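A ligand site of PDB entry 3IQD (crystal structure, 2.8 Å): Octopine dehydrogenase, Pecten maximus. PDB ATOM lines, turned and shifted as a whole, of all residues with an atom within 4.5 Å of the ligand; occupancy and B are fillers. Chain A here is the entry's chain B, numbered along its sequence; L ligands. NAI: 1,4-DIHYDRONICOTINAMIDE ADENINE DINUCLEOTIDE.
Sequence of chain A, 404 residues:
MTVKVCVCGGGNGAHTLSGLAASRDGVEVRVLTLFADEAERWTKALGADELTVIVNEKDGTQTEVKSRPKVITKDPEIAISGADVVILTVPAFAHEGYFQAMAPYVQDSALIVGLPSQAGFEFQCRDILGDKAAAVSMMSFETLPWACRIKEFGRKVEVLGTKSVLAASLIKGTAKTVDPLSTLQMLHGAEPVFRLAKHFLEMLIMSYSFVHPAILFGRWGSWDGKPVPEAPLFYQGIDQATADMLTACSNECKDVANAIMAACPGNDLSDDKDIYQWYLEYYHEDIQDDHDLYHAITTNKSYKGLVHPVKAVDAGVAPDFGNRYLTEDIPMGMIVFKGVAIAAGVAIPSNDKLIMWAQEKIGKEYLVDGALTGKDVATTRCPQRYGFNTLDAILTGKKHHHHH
The side-chain carboxylate (OE1) of Glu 38 is in hydrogen-bond range of the side-chain hydroxyl (OG1) of Thr 33 (2.7 Å).
OG1 of Thr 33 touches O2B of the ligand (3.97 Å). Phe 35 touches the ligand (CD1 to C6A, 3.5 Å). Pro 91 touches the ligand. CE2 of Phe 93 touches N6A of the ligand, 3.4 Å away. CB of Ala 94 touches N3A of the ligand, at 3.8 Å. Pro 116 touches the ligand (CD to O4D, 3.3 Å). Thr 143 touches the ligand (OG1 to C6N, 3.7 Å). Leu 144 touches the ligand (CB to C6N, 3.5 Å). Trp 146 touches the ligand. CA of Ala 147 touches N7N of the ligand (3.4 Å). Hydrophobic or aromatic side chains within 4 Å of the ligand: Phe 35, Pro 91, Phe 93, Ala 94, Pro 116 and Leu 144.
N of Gly 13 lies within hydrogen-bond range of O2N of the ligand (2.7 Å). OE2 of Glu 38 is in hydrogen-bond range of O3B of the ligand (2.8 Å). The backbone NH (N) of Asn 12 sits at hydrogen-bond distance from an oxygen (O2A) of the ligand (3.1 Å). ND2 of Asn 12 lies within hydrogen-bond range of O1N of the ligand (2.8 Å). An oxygen (O2B) of the ligand lies within hydrogen-bond range of the backbone NH (N) of Gly 10 (3.2 Å). O of Gly 10 lies close to O3B of the ligand, 3.1 Å away. The backbone carbonyl oxygen (O) of Cys 148 sits at hydrogen-bond distance from a nitrogen (N7N) of the ligand. The guanidinium group (NH1) of Arg 324 lies within salt-bridge range of an oxygen (O1A) of the ligand. N of Gly 11 is in hydrogen-bond range of O3B of the ligand.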
ATOM      1  N   GLY A   9       6.420 -28.810  14.942  1.00  0.00           N
ATOM      2  CA  GLY A   9       6.636 -27.954  16.104  1.00  0.00           C
ATOM      3  C   GLY A   9       7.987 -28.141  16.750  1.00  0.00           C
ATOM      4  O   GLY A   9       8.719 -29.077  16.409  1.00  0.00           O
ATOM      5  N   GLY A  10       8.317 -27.245  17.685  1.00  0.00           N
ATOM      6  CA  GLY A  10       9.576 -27.326  18.435  1.00  0.00           C
ATOM      7  C   GLY A  10       9.379 -27.021  19.912  1.00  0.00           C
ATOM      8  O   GLY A  10      10.325 -26.662  20.618  1.00  0.00           O
ATOM      9  N   GLY A  11       8.147 -27.168  20.388  1.00  0.00           N
ATOM     10  CA  GLY A  11       7.828 -26.912  21.787  1.00  0.00           C
ATOM     11  C   GLY A  11       8.041 -28.119  22.679  1.00  0.00           C
ATOM     12  O   GLY A  11       8.673 -29.103  22.272  1.00  0.00           O
ATOM     13  N   ASN A  12       7.541 -28.045  23.902  1.00  0.00           N
ATOM     14  CA  ASN A  12       7.595 -29.159  24.850  1.00  0.00           C
ATOM     15  C   ASN A  12       7.028 -30.437  24.234  1.00  0.00           C
ATOM     16  O   ASN A  12       7.676 -31.484  24.262  1.00  0.00           O
ATOM     17  CB  ASN A  12       6.857 -28.820  26.153  1.00  0.00           C
ATOM     18  CG  ASN A  12       7.394 -27.565  26.824  1.00  0.00           C
ATOM     19  OD1 ASN A  12       8.595 -27.441  27.075  1.00  0.00           O
ATOM     20  ND2 ASN A  12       6.490 -26.625  27.112  1.00  0.00           N
ATOM     21  N   GLY A  13       5.825 -30.339  23.673  1.00  0.00           N
ATOM     22  CA  GLY A  13       5.160 -31.481  23.062  1.00  0.00           C
ATOM     23  C   GLY A  13       5.926 -32.097  21.908  1.00  0.00           C
ATOM     24  O   GLY A  13       6.076 -33.308  21.839  1.00  0.00           O
ATOM     25  N   ALA A  14       6.406 -31.242  21.005  1.00  0.00           N
ATOM     26  CA  ALA A  14       7.173 -31.660  19.836  1.00  0.00           C
ATOM     27  C   ALA A  14       8.431 -32.425  20.235  1.00  0.00           C
ATOM     28  O   ALA A  14       8.746 -33.471  19.650  1.00  0.00           O
ATOM     29  CB  ALA A  14       7.535 -30.474  18.986  1.00  0.00           C
ATOM     30  N   THR A  33       9.579 -27.868  11.638  1.00  0.00           N
ATOM     31  CA  THR A  33       9.310 -26.637  12.359  1.00  0.00           C
ATOM     32  C   THR A  33       9.565 -25.440  11.442  1.00  0.00           C
ATOM     33  O   THR A  33      10.652 -25.297  10.890  1.00  0.00           O
ATOM     34  CB  THR A  33      10.083 -26.536  13.708  1.00  0.00           C
ATOM     35  OG1 THR A  33      10.127 -25.185  14.150  1.00  0.00           O
ATOM     36  CG2 THR A  33      11.485 -27.065  13.578  1.00  0.00           C
ATOM     37  N   PHE A  35       9.067 -22.232  12.438  1.00  0.00           N
ATOM     38  CA  PHE A  35       9.371 -21.044  13.239  1.00  0.00           C
ATOM     39  C   PHE A  35      10.784 -20.539  12.961  1.00  0.00           C
ATOM     40  O   PHE A  35      11.754 -21.003  13.569  1.00  0.00           O
ATOM     41  CB  PHE A  35       9.165 -21.308  14.735  1.00  0.00           C
ATOM     42  CG  PHE A  35       9.289 -20.084  15.594  1.00  0.00           C
ATOM     43  CD1 PHE A  35       8.841 -18.834  15.149  1.00  0.00           C
ATOM     44  CD2 PHE A  35       9.818 -20.173  16.883  1.00  0.00           C
ATOM     45  CE1 PHE A  35       8.954 -17.700  15.959  1.00  0.00           C
ATOM     46  CE2 PHE A  35       9.938 -19.038  17.705  1.00  0.00           C
ATOM     47  CZ  PHE A  35       9.495 -17.805  17.233  1.00  0.00           C
ATOM     48  N   GLU A  38      14.291 -22.375  13.791  1.00  0.00           N
ATOM     49  CA  GLU A  38      14.243 -23.297  14.917  1.00  0.00           C
ATOM     50  C   GLU A  38      14.831 -24.662  14.530  1.00  0.00           C
ATOM     51  O   GLU A  38      15.500 -25.298  15.338  1.00  0.00           O
ATOM     52  CB  GLU A  38      12.809 -23.465  15.413  1.00  0.00           C
ATOM     53  CG  GLU A  38      12.683 -24.175  16.748  1.00  0.00           C
ATOM     54  CD  GLU A  38      11.298 -24.013  17.362  1.00  0.00           C
ATOM     55  OE1 GLU A  38      10.306 -24.479  16.756  1.00  0.00           O
ATOM     56  OE2 GLU A  38      11.197 -23.427  18.469  1.00  0.00           O
ATOM     57  N   THR A  89       1.931 -30.541  16.898  1.00  0.00           N
ATOM     58  CA  THR A  89       2.014 -30.264  18.335  1.00  0.00           C
ATOM     59  C   THR A  89       2.614 -28.877  18.565  1.00  0.00           C
ATOM     60  O   THR A  89       3.811 -28.724  18.815  1.00  0.00           O
ATOM     61  CB  THR A  89       2.763 -31.372  19.095  1.00  0.00           C
ATOM     62  OG1 THR A  89       2.068 -32.604  18.908  1.00  0.00           O
ATOM     63  CG2 THR A  89       2.798 -31.082  20.569  1.00  0.00           C
ATOM     64  N   VAL A  90       1.745 -27.870  18.437  1.00  0.00           N
ATOM     65  CA  VAL A  90       2.103 -26.464  18.566  1.00  0.00           C
ATOM     66  C   VAL A  90       0.885 -25.694  19.056  1.00  0.00           C
ATOM     67  O   VAL A  90      -0.246 -26.147  18.855  1.00  0.00           O
ATOM     68  CB  VAL A  90       2.517 -25.841  17.192  1.00  0.00           C
ATOM     69  CG1 VAL A  90       3.979 -26.076  16.900  1.00  0.00           C
ATOM     70  CG2 VAL A  90       1.617 -26.344  16.053  1.00  0.00           C
ATOM     71  N   PRO A  91       1.104 -24.533  19.694  1.00  0.00           N
ATOM     72  CA  PRO A  91      -0.009 -23.620  19.968  1.00  0.00           C
ATOM     73  C   PRO A  91      -0.834 -23.389  18.690  1.00  0.00           C
ATOM     74  O   PRO A  91      -0.278 -23.189  17.611  1.00  0.00           O
ATOM     75  CB  PRO A  91       0.692 -22.323  20.388  1.00  0.00           C
ATOM     76  CG  PRO A  91       1.982 -22.775  20.967  1.00  0.00           C
ATOM     77  CD  PRO A  91       2.378 -24.018  20.226  1.00  0.00           C
ATOM     78  N   PHE A  93      -2.243 -21.186  17.056  1.00  0.00           N
ATOM     79  CA  PHE A  93      -1.985 -20.087  16.123  1.00  0.00           C
ATOM     80  C   PHE A  93      -0.947 -20.458  15.055  1.00  0.00           C
ATOM     81  O   PHE A  93      -0.905 -19.844  13.985  1.00  0.00           O
ATOM     82  CB  PHE A  93      -1.606 -18.785  16.855  1.00  0.00           C
ATOM     83  CG  PHE A  93      -0.204 -18.771  17.404  1.00  0.00           C
ATOM     84  CD1 PHE A  93       0.019 -18.989  18.766  1.00  0.00           C
ATOM     85  CD2 PHE A  93       0.886 -18.495  16.575  1.00  0.00           C
ATOM     86  CE1 PHE A  93       1.315 -18.962  19.289  1.00  0.00           C
ATOM     87  CE2 PHE A  93       2.180 -18.475  17.091  1.00  0.00           C
ATOM     88  CZ  PHE A  93       2.403 -18.704  18.463  1.00  0.00           C
ATOM     89  N   ALA A  94      -0.124 -21.458  15.353  1.00  0.00           N
ATOM     90  CA  ALA A  94       0.881 -21.960  14.421  1.00  0.00           C
ATOM     91  C   ALA A  94       0.318 -22.952  13.402  1.00  0.00           C
ATOM     92  O   ALA A  94       0.985 -23.279  12.411  1.00  0.00           O
ATOM     93  CB  ALA A  94       2.033 -22.595  15.176  1.00  0.00           C
ATOM     94  N   TYR A  98       1.469 -24.613   9.164  1.00  0.00           N
ATOM     95  CA  TYR A  98       1.770 -26.004   8.844  1.00  0.00           C
ATOM     96  C   TYR A  98       0.836 -26.566   7.783  1.00  0.00           C
ATOM     97  O   TYR A  98       1.294 -27.246   6.864  1.00  0.00           O
ATOM     98  CB  TYR A  98       1.772 -26.886  10.092  1.00  0.00           C
ATOM     99  CG  TYR A  98       2.906 -26.543  11.018  1.00  0.00           C
ATOM    100  CD1 TYR A  98       4.212 -26.955  10.726  1.00  0.00           C
ATOM    101  CD2 TYR A  98       2.699 -25.774  12.155  1.00  0.00           C
ATOM    102  CE1 TYR A  98       5.273 -26.614  11.563  1.00  0.00           C
ATOM    103  CE2 TYR A  98       3.752 -25.436  12.997  1.00  0.00           C
ATOM    104  CZ  TYR A  98       5.029 -25.853  12.699  1.00  0.00           C
ATOM    105  OH  TYR A  98       6.069 -25.504  13.532  1.00  0.00           O
ATOM    106  N   PRO A 116      -2.387 -31.143  20.803  1.00  0.00           N
ATOM    107  CA  PRO A 116      -3.843 -31.158  20.733  1.00  0.00           C
ATOM    108  C   PRO A 116      -4.352 -30.357  19.536  1.00  0.00           C
ATOM    109  O   PRO A 116      -3.572 -29.661  18.881  1.00  0.00           O
ATOM    110  CB  PRO A 116      -4.248 -30.462  22.028  1.00  0.00           C
ATOM    111  CG  PRO A 116      -3.175 -29.477  22.256  1.00  0.00           C
ATOM    112  CD  PRO A 116      -1.910 -30.075  21.701  1.00  0.00           C
ATOM    113  N   THR A 143      -6.481 -32.981  24.571  1.00  0.00           N
ATOM    114  CA  THR A 143      -5.397 -32.208  25.168  1.00  0.00           C
ATOM    115  C   THR A 143      -4.058 -32.886  24.869  1.00  0.00           C
ATOM    116  O   THR A 143      -4.015 -33.860  24.119  1.00  0.00           O
ATOM    117  CB  THR A 143      -5.633 -32.001  26.706  1.00  0.00           C
ATOM    118  OG1 THR A 143      -4.662 -31.086  27.233  1.00  0.00           O
ATOM    119  CG2 THR A 143      -5.548 -33.305  27.470  1.00  0.00           C
ATOM    120  N   LEU A 144      -2.969 -32.379  25.434  1.00  0.00           N
ATOM    121  CA  LEU A 144      -1.672 -33.010  25.265  1.00  0.00           C
ATOM    122  C   LEU A 144      -1.528 -34.210  26.216  1.00  0.00           C
ATOM    123  O   LEU A 144      -1.818 -34.102  27.404  1.00  0.00           O
ATOM    124  CB  LEU A 144      -0.539 -32.001  25.503  1.00  0.00           C
ATOM    125  CG  LEU A 144       0.882 -32.383  25.093  1.00  0.00           C
ATOM    126  CD1 LEU A 144       1.072 -32.317  23.571  1.00  0.00           C
ATOM    127  CD2 LEU A 144       1.884 -31.482  25.788  1.00  0.00           C
ATOM    128  N   TRP A 146       0.871 -35.532  27.723  1.00  0.00           N
ATOM    129  CA  TRP A 146       1.788 -35.380  28.857  1.00  0.00           C
ATOM    130  C   TRP A 146       1.742 -33.974  29.442  1.00  0.00           C
ATOM    131  O   TRP A 146       1.318 -33.028  28.772  1.00  0.00           O
ATOM    132  CB  TRP A 146       3.231 -35.689  28.442  1.00  0.00           C
ATOM    133  CG  TRP A 146       3.344 -36.739  27.388  1.00  0.00           C
ATOM    134  CD1 TRP A 146       3.384 -38.085  27.572  1.00  0.00           C
ATOM    135  CD2 TRP A 146       3.411 -36.526  25.977  1.00  0.00           C
ATOM    136  NE1 TRP A 146       3.484 -38.725  26.363  1.00  0.00           N
ATOM    137  CE2 TRP A 146       3.494 -37.787  25.369  1.00  0.00           C
ATOM    138  CE3 TRP A 146       3.398 -35.386  25.168  1.00  0.00           C
ATOM    139  CZ2 TRP A 146       3.588 -37.956  23.984  1.00  0.00           C
ATOM    140  CZ3 TRP A 146       3.488 -35.535  23.793  1.00  0.00           C
ATOM    141  CH2 TRP A 146       3.577 -36.814  23.216  1.00  0.00           C
ATOM    142  N   ALA A 147       2.172 -33.865  30.688  1.00  0.00           N
ATOM    143  CA  ALA A 147       2.601 -32.600  31.249  1.00  0.00           C
ATOM    144  C   ALA A 147       4.113 -32.609  31.093  1.00  0.00           C
ATOM    145  O   ALA A 147       4.810 -33.408  31.734  1.00  0.00           O
ATOM    146  CB  ALA A 147       2.195 -32.493  32.712  1.00  0.00           C
ATOM    147  N   CYS A 148       4.628 -31.758  30.218  1.00  0.00           N
ATOM    148  CA  CYS A 148       6.056 -31.781  29.873  1.00  0.00           C
ATOM    149  C   CYS A 148       6.719 -30.408  29.779  1.00  0.00           C
ATOM    150  O   CYS A 148       6.070 -29.395  29.529  1.00  0.00           O
ATOM    151  CB  CYS A 148       6.273 -32.568  28.581  1.00  0.00           C
ATOM    152  SG  CYS A 148       5.261 -32.025  27.185  1.00  0.00           S
ATOM    153  N   ARG A 324      -2.759 -17.617  27.879  1.00  0.00           N
ATOM    154  CA  ARG A 324      -3.287 -18.487  26.832  1.00  0.00           C
ATOM    155  C   ARG A 324      -4.672 -19.010  27.194  1.00  0.00           C
ATOM    156  O   ARG A 324      -5.357 -19.610  26.367  1.00  0.00           O
ATOM    157  CB  ARG A 324      -2.315 -19.622  26.488  1.00  0.00           C
ATOM    158  CG  ARG A 324      -1.268 -19.184  25.458  1.00  0.00           C
ATOM    159  CD  ARG A 324      -0.136 -20.194  25.251  1.00  0.00           C
ATOM    160  NE  ARG A 324       0.998 -19.562  24.556  1.00  0.00           N
ATOM    161  CZ  ARG A 324       2.067 -20.205  24.087  1.00  0.00           C
ATOM    162  NH1 ARG A 324       2.174 -21.522  24.218  1.00  0.00           N
ATOM    163  NH2 ARG A 324       3.023 -19.523  23.465  1.00  0.00           N
ATOM    164  N   GLU A 328      -5.877 -18.052  23.462  1.00  0.00           N
ATOM    165  CA  GLU A 328      -6.117 -19.322  22.765  1.00  0.00           C
ATOM    166  C   GLU A 328      -7.550 -19.804  22.935  1.00  0.00           C
ATOM    167  O   GLU A 328      -8.245 -20.031  21.946  1.00  0.00           O
ATOM    168  CB  GLU A 328      -5.143 -20.402  23.237  1.00  0.00           C
ATOM    169  CG  GLU A 328      -3.787 -20.378  22.554  1.00  0.00           C
ATOM    170  CD  GLU A 328      -3.578 -21.534  21.594  1.00  0.00           C
ATOM    171  OE1 GLU A 328      -2.865 -21.346  20.576  1.00  0.00           O
ATOM    172  OE2 GLU A 328      -4.135 -22.637  21.843  1.00  0.00           O
HETATM  173  PA  NAI L   1       5.073 -24.601  23.303  1.00  0.00           P
HETATM  174  O1A NAI L   1       4.710 -23.280  23.845  1.00  0.00           O
HETATM  175  O2A NAI L   1       6.205 -25.225  24.035  1.00  0.00           O
HETATM  176  O5B NAI L   1       5.421 -24.452  21.747  1.00  0.00           O
HETATM  177  C5B NAI L   1       6.310 -23.457  21.275  1.00  0.00           C
HETATM  178  C4B NAI L   1       6.442 -23.710  19.783  1.00  0.00           C
HETATM  179  O4B NAI L   1       5.450 -22.990  19.077  1.00  0.00           O
HETATM  180  C3B NAI L   1       7.764 -23.259  19.216  1.00  0.00           C
HETATM  181  O3B NAI L   1       8.724 -24.272  19.337  1.00  0.00           O
HETATM  182  C2B NAI L   1       7.417 -22.988  17.775  1.00  0.00           C
HETATM  183  O2B NAI L   1       7.571 -24.161  17.011  1.00  0.00           O
HETATM  184  C1B NAI L   1       5.949 -22.574  17.816  1.00  0.00           C
HETATM  185  N9A NAI L   1       5.853 -21.105  17.687  1.00  0.00           N
HETATM  186  C8A NAI L   1       5.982 -20.175  18.686  1.00  0.00           C
HETATM  187  N7A NAI L   1       5.844 -18.937  18.138  1.00  0.00           N
HETATM  188  C5A NAI L   1       5.637 -19.068  16.813  1.00  0.00           C
HETATM  189  C6A NAI L   1       5.425 -18.137  15.801  1.00  0.00           C
HETATM  190  N6A NAI L   1       5.026 -16.912  16.117  1.00  0.00           N
HETATM  191  N1A NAI L   1       5.233 -18.578  14.501  1.00  0.00           N
HETATM  192  C2A NAI L   1       5.240 -19.941  14.221  1.00  0.00           C
HETATM  193  N3A NAI L   1       5.447 -20.859  15.236  1.00  0.00           N
HETATM  194  C4A NAI L   1       5.644 -20.428  16.516  1.00  0.00           C
HETATM  195  O3  NAI L   1       3.785 -25.574  23.293  1.00  0.00           O
HETATM  196  PN  NAI L   1       3.775 -27.013  24.007  1.00  0.00           P
HETATM  197  O1N NAI L   1       4.229 -26.849  25.407  1.00  0.00           O
HETATM  198  O2N NAI L   1       4.451 -28.030  23.156  1.00  0.00           O
HETATM  199  O5D NAI L   1       2.198 -27.299  24.028  1.00  0.00           O
HETATM  200  C5D NAI L   1       1.504 -27.537  22.820  1.00  0.00           C
HETATM  201  C4D NAI L   1       0.011 -27.311  23.041  1.00  0.00           C
HETATM  202  O4D NAI L   1      -0.460 -28.227  24.004  1.00  0.00           O
HETATM  203  C3D NAI L   1      -0.264 -25.909  23.562  1.00  0.00           C
HETATM  204  O3D NAI L   1      -1.364 -25.384  22.854  1.00  0.00           O
HETATM  205  C2D NAI L   1      -0.618 -26.092  25.024  1.00  0.00           C
HETATM  206  O2D NAI L   1      -1.679 -25.233  25.388  1.00  0.00           O
HETATM  207  C1D NAI L   1      -1.028 -27.558  25.120  1.00  0.00           C
HETATM  208  N1N NAI L   1      -0.630 -28.215  26.387  1.00  0.00           N
HETATM  209  C2N NAI L   1       0.624 -28.061  26.931  1.00  0.00           C
HETATM  210  C3N NAI L   1       0.959 -28.705  28.136  1.00  0.00           C
HETATM  211  C7N NAI L   1       2.398 -28.945  28.480  1.00  0.00           C
HETATM  212  O7N NAI L   1       3.429 -28.383  27.698  1.00  0.00           O
HETATM  213  N7N NAI L   1       2.686 -29.717  29.536  1.00  0.00           N
HETATM  214  C4N NAI L   1      -0.009 -29.489  28.776  1.00  0.00           C
HETATM  215  C5N NAI L   1      -1.270 -29.644  28.221  1.00  0.00           C
HETATM  216  C6N NAI L   1      -1.568 -28.992  27.017  1.00  0.00           C
